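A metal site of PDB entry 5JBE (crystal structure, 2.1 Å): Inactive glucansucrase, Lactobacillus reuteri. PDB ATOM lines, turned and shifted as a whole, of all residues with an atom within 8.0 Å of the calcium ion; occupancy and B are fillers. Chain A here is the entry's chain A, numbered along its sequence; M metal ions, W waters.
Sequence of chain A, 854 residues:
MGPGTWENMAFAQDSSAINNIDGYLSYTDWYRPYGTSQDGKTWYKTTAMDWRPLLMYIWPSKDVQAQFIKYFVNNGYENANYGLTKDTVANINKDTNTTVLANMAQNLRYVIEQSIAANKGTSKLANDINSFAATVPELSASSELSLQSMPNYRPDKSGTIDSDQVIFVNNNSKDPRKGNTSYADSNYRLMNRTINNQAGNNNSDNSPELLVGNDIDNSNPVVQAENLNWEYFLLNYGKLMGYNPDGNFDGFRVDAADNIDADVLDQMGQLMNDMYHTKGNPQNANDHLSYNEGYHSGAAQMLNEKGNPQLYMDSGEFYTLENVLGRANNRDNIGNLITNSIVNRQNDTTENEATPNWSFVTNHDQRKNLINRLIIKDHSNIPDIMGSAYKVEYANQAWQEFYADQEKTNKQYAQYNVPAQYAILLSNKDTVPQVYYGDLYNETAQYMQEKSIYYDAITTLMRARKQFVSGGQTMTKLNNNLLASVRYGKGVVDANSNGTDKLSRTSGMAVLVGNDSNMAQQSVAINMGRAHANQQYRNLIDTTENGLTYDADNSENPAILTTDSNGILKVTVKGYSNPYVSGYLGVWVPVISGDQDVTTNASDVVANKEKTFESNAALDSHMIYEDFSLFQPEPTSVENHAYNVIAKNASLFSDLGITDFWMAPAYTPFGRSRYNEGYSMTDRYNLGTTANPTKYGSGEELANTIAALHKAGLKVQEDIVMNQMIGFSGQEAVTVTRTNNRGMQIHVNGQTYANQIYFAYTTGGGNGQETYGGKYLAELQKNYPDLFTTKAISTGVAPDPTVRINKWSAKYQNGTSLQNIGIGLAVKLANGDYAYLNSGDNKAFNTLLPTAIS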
ATOM      1  N   LEU A 190     -16.139 -10.936 -23.871  1.00  0.00           N
ATOM      2  CA  LEU A 190     -15.897 -12.392 -23.776  1.00  0.00           C
ATOM      3  C   LEU A 190     -14.469 -12.540 -23.283  1.00  0.00           C
ATOM      4  O   LEU A 190     -13.533 -12.262 -24.030  1.00  0.00           O
ATOM      5  CB  LEU A 190     -16.113 -13.117 -25.104  1.00  0.00           C
ATOM      6  CG  LEU A 190     -17.472 -12.897 -25.788  1.00  0.00           C
ATOM      7  CD1 LEU A 190     -17.564 -13.749 -27.037  1.00  0.00           C
ATOM      8  CD2 LEU A 190     -18.632 -13.213 -24.850  1.00  0.00           C
ATOM      9  N   MET A 191     -14.316 -12.925 -22.015  1.00  0.00           N
ATOM     10  CA  MET A 191     -12.998 -13.057 -21.387  1.00  0.00           C
ATOM     11  C   MET A 191     -12.498 -14.511 -21.391  1.00  0.00           C
ATOM     12  O   MET A 191     -13.279 -15.435 -21.369  1.00  0.00           O
ATOM     13  CB  MET A 191     -13.012 -12.539 -19.944  1.00  0.00           C
ATOM     14  CG  MET A 191     -13.230 -11.023 -19.874  1.00  0.00           C
ATOM     15  SD  MET A 191     -13.237 -10.403 -18.188  1.00  0.00           S
ATOM     16  CE  MET A 191     -11.541 -10.682 -17.671  1.00  0.00           C
ATOM     17  N   ASN A 192     -11.173 -14.643 -21.471  1.00  0.00           N
ATOM     18  CA  ASN A 192     -10.470 -15.934 -21.428  1.00  0.00           C
ATOM     19  C   ASN A 192     -10.775 -16.826 -22.640  1.00  0.00           C
ATOM     20  O   ASN A 192     -10.717 -18.034 -22.527  1.00  0.00           O
ATOM     21  CB  ASN A 192     -10.765 -16.693 -20.110  1.00  0.00           C
ATOM     22  CG  ASN A 192     -10.645 -15.804 -18.879  1.00  0.00           C
ATOM     23  OD1 ASN A 192      -9.558 -15.382 -18.524  1.00  0.00           O
ATOM     24  ND2 ASN A 192     -11.733 -15.562 -18.201  1.00  0.00           N
ATOM     25  N   THR A 194      -8.935 -17.677 -24.848  1.00  0.00           N
ATOM     26  CA  THR A 194      -7.508 -17.668 -25.039  1.00  0.00           C
ATOM     27  C   THR A 194      -7.060 -19.066 -25.429  1.00  0.00           C
ATOM     28  O   THR A 194      -7.531 -20.070 -24.873  1.00  0.00           O
ATOM     29  CB  THR A 194      -6.817 -17.206 -23.735  1.00  0.00           C
ATOM     30  OG1 THR A 194      -7.347 -17.936 -22.602  1.00  0.00           O
ATOM     31  CG2 THR A 194      -7.054 -15.709 -23.520  1.00  0.00           C
ATOM     32  N   PRO A 208      -4.907 -16.834 -18.708  1.00  0.00           N
ATOM     33  CA  PRO A 208      -5.713 -15.708 -18.200  1.00  0.00           C
ATOM     34  C   PRO A 208      -5.880 -14.525 -19.155  1.00  0.00           C
ATOM     35  O   PRO A 208      -4.979 -14.197 -19.926  1.00  0.00           O
ATOM     36  CB  PRO A 208      -4.921 -15.272 -16.970  1.00  0.00           C
ATOM     37  CG  PRO A 208      -3.496 -15.595 -17.332  1.00  0.00           C
ATOM     38  CD  PRO A 208      -3.583 -16.891 -18.066  1.00  0.00           C
ATOM     39  N   GLU A 209      -7.035 -13.882 -19.061  1.00  0.00           N
ATOM     40  CA  GLU A 209      -7.328 -12.660 -19.822  1.00  0.00           C
ATOM     41  C   GLU A 209      -6.512 -11.475 -19.344  1.00  0.00           C
ATOM     42  O   GLU A 209      -6.091 -10.614 -20.142  1.00  0.00           O
ATOM     43  CB  GLU A 209      -8.809 -12.321 -19.720  1.00  0.00           C
ATOM     44  CG  GLU A 209      -9.255 -11.121 -20.587  1.00  0.00           C
ATOM     45  CD  GLU A 209      -9.020 -11.347 -22.079  1.00  0.00           C
ATOM     46  OE1 GLU A 209      -9.621 -12.321 -22.615  1.00  0.00           O
ATOM     47  OE2 GLU A 209      -8.243 -10.545 -22.689  1.00  0.00           O
ATOM     48  N   LEU A 210      -6.282 -11.398 -18.042  1.00  0.00           N
ATOM     49  CA  LEU A 210      -5.689 -10.199 -17.449  1.00  0.00           C
ATOM     50  C   LEU A 210      -4.237 -10.392 -17.063  1.00  0.00           C
ATOM     51  O   LEU A 210      -3.895 -11.409 -16.481  1.00  0.00           O
ATOM     52  CB  LEU A 210      -6.509  -9.780 -16.245  1.00  0.00           C
ATOM     53  CG  LEU A 210      -7.987  -9.539 -16.506  1.00  0.00           C
ATOM     54  CD1 LEU A 210      -8.689  -9.084 -15.224  1.00  0.00           C
ATOM     55  CD2 LEU A 210      -8.220  -8.533 -17.626  1.00  0.00           C
ATOM     56  N   LEU A 211      -3.396  -9.401 -17.417  1.00  0.00           N
ATOM     57  CA  LEU A 211      -2.001  -9.312 -17.005  1.00  0.00           C
ATOM     58  C   LEU A 211      -1.790  -8.052 -16.164  1.00  0.00           C
ATOM     59  O   LEU A 211      -1.721  -8.136 -14.933  1.00  0.00           O
ATOM     60  CB  LEU A 211      -1.052  -9.282 -18.212  1.00  0.00           C
ATOM     61  CG  LEU A 211      -0.957 -10.480 -19.122  1.00  0.00           C
ATOM     62  CD1 LEU A 211       0.205 -10.230 -20.092  1.00  0.00           C
ATOM     63  CD2 LEU A 211      -0.735 -11.769 -18.331  1.00  0.00           C
ATOM     64  N   VAL A 212      -1.718  -6.896 -16.823  1.00  0.00           N
ATOM     65  CA  VAL A 212      -1.488  -5.624 -16.162  1.00  0.00           C
ATOM     66  C   VAL A 212      -2.010  -4.509 -17.096  1.00  0.00           C
ATOM     67  O   VAL A 212      -2.109  -4.727 -18.292  1.00  0.00           O
ATOM     68  CB  VAL A 212       0.009  -5.420 -15.831  1.00  0.00           C
ATOM     69  CG1 VAL A 212       0.840  -5.238 -17.092  1.00  0.00           C
ATOM     70  CG2 VAL A 212       0.224  -4.250 -14.882  1.00  0.00           C
ATOM     71  N   ASN A 214      -4.785  -1.389 -18.484  1.00  0.00           N
ATOM     72  CA  ASN A 214      -6.157  -1.422 -18.967  1.00  0.00           C
ATOM     73  C   ASN A 214      -6.263  -2.493 -20.010  1.00  0.00           C
ATOM     74  O   ASN A 214      -5.685  -2.361 -21.108  1.00  0.00           O
ATOM     75  CB  ASN A 214      -6.575  -0.098 -19.582  1.00  0.00           C
ATOM     76  CG  ASN A 214      -6.660   1.022 -18.566  1.00  0.00           C
ATOM     77  OD1 ASN A 214      -5.633   1.504 -18.090  1.00  0.00           O
ATOM     78  ND2 ASN A 214      -7.871   1.444 -18.243  1.00  0.00           N
ATOM     79  N   ASP A 215      -7.003  -3.559 -19.697  1.00  0.00           N
ATOM     80  CA  ASP A 215      -7.112  -4.710 -20.611  1.00  0.00           C
ATOM     81  C   ASP A 215      -8.089  -4.411 -21.767  1.00  0.00           C
ATOM     82  O   ASP A 215      -9.270  -4.103 -21.508  1.00  0.00           O
ATOM     83  CB  ASP A 215      -7.576  -5.939 -19.853  1.00  0.00           C
ATOM     84  CG  ASP A 215      -7.322  -7.226 -20.609  1.00  0.00           C
ATOM     85  OD1 ASP A 215      -6.140  -7.653 -20.666  1.00  0.00           O
ATOM     86  OD2 ASP A 215      -8.284  -7.816 -21.143  1.00  0.00           O
ATOM     87  N   ILE A 216      -7.620  -4.518 -23.007  1.00  0.00           N
ATOM     88  CA  ILE A 216      -8.469  -4.222 -24.176  1.00  0.00           C
ATOM     89  C   ILE A 216      -9.418  -5.392 -24.467  1.00  0.00           C
ATOM     90  O   ILE A 216      -8.996  -6.569 -24.450  1.00  0.00           O
ATOM     91  CB  ILE A 216      -7.604  -3.942 -25.427  1.00  0.00           C
ATOM     92  CG1 ILE A 216      -6.674  -2.748 -25.195  1.00  0.00           C
ATOM     93  CG2 ILE A 216      -8.479  -3.744 -26.659  1.00  0.00           C
ATOM     94  CD1 ILE A 216      -7.352  -1.417 -24.916  1.00  0.00           C
ATOM     95  N   ASP A 217     -10.675  -5.082 -24.765  1.00  0.00           N
ATOM     96  CA  ASP A 217     -11.643  -6.133 -25.112  1.00  0.00           C
ATOM     97  C   ASP A 217     -11.493  -6.571 -26.585  1.00  0.00           C
ATOM     98  O   ASP A 217     -12.209  -6.081 -27.461  1.00  0.00           O
ATOM     99  CB  ASP A 217     -13.080  -5.722 -24.805  1.00  0.00           C
ATOM    100  CG  ASP A 217     -14.076  -6.797 -25.147  1.00  0.00           C
ATOM    101  OD1 ASP A 217     -13.669  -7.975 -25.349  1.00  0.00           O
ATOM    102  OD2 ASP A 217     -15.276  -6.493 -25.218  1.00  0.00           O
ATOM    103  N   ASN A 218     -10.590  -7.528 -26.826  1.00  0.00           N
ATOM    104  CA  ASN A 218     -10.359  -8.057 -28.176  1.00  0.00           C
ATOM    105  C   ASN A 218     -11.435  -9.015 -28.711  1.00  0.00           C
ATOM    106  O   ASN A 218     -11.282  -9.558 -29.819  1.00  0.00           O
ATOM    107  CB  ASN A 218      -8.957  -8.676 -28.280  1.00  0.00           C
ATOM    108  CG  ASN A 218      -7.847  -7.646 -28.167  1.00  0.00           C
ATOM    109  OD1 ASN A 218      -7.671  -6.825 -29.064  1.00  0.00           O
ATOM    110  ND2 ASN A 218      -7.110  -7.660 -27.055  1.00  0.00           N
ATOM    111  N   ALA A 256       1.853 -10.979 -25.844  1.00  0.00           N
ATOM    112  CA  ALA A 256       0.794 -11.539 -24.993  1.00  0.00           C
ATOM    113  C   ALA A 256      -0.245 -12.342 -25.779  1.00  0.00           C
ATOM    114  O   ALA A 256      -1.455 -12.243 -25.522  1.00  0.00           O
ATOM    115  CB  ALA A 256       0.129 -10.408 -24.203  1.00  0.00           C
ATOM    116  N   ASP A 258      -1.120 -15.336 -25.599  1.00  0.00           N
ATOM    117  CA  ASP A 258      -1.890 -16.235 -24.738  1.00  0.00           C
ATOM    118  C   ASP A 258      -2.981 -15.517 -23.908  1.00  0.00           C
ATOM    119  O   ASP A 258      -3.781 -16.187 -23.244  1.00  0.00           O
ATOM    120  CB  ASP A 258      -0.958 -16.976 -23.760  1.00  0.00           C
ATOM    121  CG  ASP A 258       0.066 -17.889 -24.473  1.00  0.00           C
ATOM    122  OD1 ASP A 258      -0.047 -18.114 -25.704  1.00  0.00           O
ATOM    123  OD2 ASP A 258       0.977 -18.370 -23.759  1.00  0.00           O
ATOM    124  N   ASN A 259      -3.013 -14.185 -23.946  1.00  0.00           N
ATOM    125  CA  ASN A 259      -3.866 -13.402 -23.035  1.00  0.00           C
ATOM    126  C   ASN A 259      -4.869 -12.498 -23.743  1.00  0.00           C
ATOM    127  O   ASN A 259      -5.438 -11.618 -23.127  1.00  0.00           O
ATOM    128  CB  ASN A 259      -3.001 -12.560 -22.109  1.00  0.00           C
ATOM    129  CG  ASN A 259      -1.912 -13.366 -21.443  1.00  0.00           C
ATOM    130  OD1 ASN A 259      -0.735 -13.151 -21.738  1.00  0.00           O
ATOM    131  ND2 ASN A 259      -2.286 -14.317 -20.577  1.00  0.00           N
ATOM    132  N   ILE A 260      -5.136 -12.757 -25.024  1.00  0.00           N
ATOM    133  CA  ILE A 260      -6.079 -11.974 -25.828  1.00  0.00           C
ATOM    134  C   ILE A 260      -7.008 -12.948 -26.550  1.00  0.00           C
ATOM    135  O   ILE A 260      -6.591 -14.080 -26.833  1.00  0.00           O
ATOM    136  CB  ILE A 260      -5.311 -11.089 -26.852  1.00  0.00           C
ATOM    137  CG1 ILE A 260      -4.388 -11.937 -27.753  1.00  0.00           C
ATOM    138  CG2 ILE A 260      -4.510 -10.012 -26.120  1.00  0.00           C
ATOM    139  CD1 ILE A 260      -3.467 -11.147 -28.670  1.00  0.00           C
ATOM    140  N   ASP A 261      -8.228 -12.513 -26.869  1.00  0.00           N
ATOM    141  CA  ASP A 261      -9.153 -13.323 -27.685  1.00  0.00           C
ATOM    142  C   ASP A 261      -8.423 -13.851 -28.950  1.00  0.00           C
ATOM    143  O   ASP A 261      -7.930 -13.079 -29.775  1.00  0.00           O
ATOM    144  CB  ASP A 261     -10.400 -12.505 -28.045  1.00  0.00           C
ATOM    145  CG  ASP A 261     -11.546 -13.352 -28.576  1.00  0.00           C
ATOM    146  OD1 ASP A 261     -11.278 -14.320 -29.323  1.00  0.00           O
ATOM    147  OD2 ASP A 261     -12.735 -13.018 -28.293  1.00  0.00           O
ATOM    148  N   MET A 722      -1.621  -5.854 -28.563  1.00  0.00           N
ATOM    149  CA  MET A 722      -3.088  -5.765 -28.460  1.00  0.00           C
ATOM    150  C   MET A 722      -3.683  -5.915 -27.039  1.00  0.00           C
ATOM    151  O   MET A 722      -4.869  -5.686 -26.852  1.00  0.00           O
ATOM    152  CB  MET A 722      -3.755  -6.773 -29.409  1.00  0.00           C
ATOM    153  CG  MET A 722      -3.562  -6.419 -30.886  1.00  0.00           C
ATOM    154  SD  MET A 722      -4.266  -7.621 -32.042  1.00  0.00           S
ATOM    155  CE  MET A 722      -2.957  -8.837 -32.115  1.00  0.00           C
ATOM    156  N   ASN A 723      -2.886  -6.322 -26.042  1.00  0.00           N
ATOM    157  CA  ASN A 723      -3.476  -6.742 -24.788  1.00  0.00           C
ATOM    158  C   ASN A 723      -3.966  -5.598 -23.914  1.00  0.00           C
ATOM    159  O   ASN A 723      -5.059  -5.699 -23.334  1.00  0.00           O
ATOM    160  CB  ASN A 723      -2.498  -7.581 -23.953  1.00  0.00           C
ATOM    161  CG  ASN A 723      -3.152  -8.047 -22.662  1.00  0.00           C
ATOM    162  OD1 ASN A 723      -4.031  -8.902 -22.675  1.00  0.00           O
ATOM    163  ND2 ASN A 723      -2.760  -7.451 -21.543  1.00  0.00           N
ATOM    164  N   GLN A 724      -3.107  -4.597 -23.725  1.00  0.00           N
ATOM    165  CA  GLN A 724      -3.359  -3.494 -22.799  1.00  0.00           C
ATOM    166  C   GLN A 724      -2.832  -2.164 -23.311  1.00  0.00           C
ATOM    167  O   GLN A 724      -1.916  -2.131 -24.136  1.00  0.00           O
ATOM    168  CB  GLN A 724      -2.778  -3.761 -21.408  1.00  0.00           C
ATOM    169  CG  GLN A 724      -1.291  -3.458 -21.205  1.00  0.00           C
ATOM    170  CD  GLN A 724      -0.361  -4.485 -21.849  1.00  0.00           C
ATOM    171  OE1 GLN A 724      -0.619  -5.688 -21.823  1.00  0.00           O
ATOM    172  NE2 GLN A 724       0.732  -4.017 -22.431  1.00  0.00           N
ATOM    173  N   ASN A 741      -7.041 -12.843 -12.148  1.00  0.00           N
ATOM    174  CA  ASN A 741      -6.659 -12.604 -13.547  1.00  0.00           C
ATOM    175  C   ASN A 741      -7.569 -13.230 -14.615  1.00  0.00           C
ATOM    176  O   ASN A 741      -7.377 -12.970 -15.811  1.00  0.00           O
ATOM    177  CB  ASN A 741      -5.202 -12.975 -13.803  1.00  0.00           C
ATOM    178  CG  ASN A 741      -4.940 -14.477 -13.668  1.00  0.00           C
ATOM    179  OD1 ASN A 741      -5.830 -15.242 -13.300  1.00  0.00           O
ATOM    180  ND2 ASN A 741      -3.715 -14.884 -13.964  1.00  0.00           N
ATOM    181  N   ASN A 814     -11.962  -4.640 -20.958  1.00  0.00           N
ATOM    182  CA  ASN A 814     -12.416  -5.705 -20.022  1.00  0.00           C
ATOM    183  C   ASN A 814     -12.289  -5.307 -18.550  1.00  0.00           C
ATOM    184  O   ASN A 814     -13.093  -5.731 -17.715  1.00  0.00           O
ATOM    185  CB  ASN A 814     -11.606  -6.992 -20.230  1.00  0.00           C
ATOM    186  CG  ASN A 814     -11.951  -7.699 -21.518  1.00  0.00           C
ATOM    187  OD1 ASN A 814     -13.105  -7.673 -21.965  1.00  0.00           O
ATOM    188  ND2 ASN A 814     -10.958  -8.377 -22.112  1.00  0.00           N
HETATM  189 CA    CA M   1      -6.305  -9.513 -22.127  1.00  0.00          CA
HETATM  190  O   HOH W   1      -6.709  -7.916 -23.905  1.00  0.00           O
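The calcium ion is bound by OE2 of Glu 209 (2.3 Å), O of Glu 209 (2.3 Å), OD1 of Asp 215 (2.4 Å), OD1 of Asn 723 (2.4 Å), water W1 (2.4 Å), O of Asn 259 (2.5 Å) and OD2 of Asp 215 (2.8 Å).
Water W1 lies within hydrogen-bond range of the backbone carbonyl oxygen of Ile 216 (2.7 Å), the backbone carbonyl oxygen of Asn 723 (2.8 Å) and the side-chain amide nitrogen of Asn 218 (3.2 Å).
O of Asp 215 lies within hydrogen-bond range of N of Asn 814 (2.8 Å). ND2 of Asn 259 lies within hydrogen-bond range of O of Pro 208, at 2.8 Å. N of Glu 209 sits at hydrogen-bond distance from O of Asn 741 (3.4 Å). The backbone NH (N) of Glu 209 is in hydrogen-bond range of the side-chain amide oxygen (OD1) of Asn 192 (3.0 Å). ND2 of Asn 723 is in hydrogen-bond range of OE1 of Gln 724, 2.8 Å away. The backbone carbonyl oxygen (O) of Asn 723 is in hydrogen-bond range of the backbone NH (N) of Ile 216.
Four residues have an atom within 4 Å of the calcium ion: Glu 209, Asp 215, Asn 259 and Asn 723.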
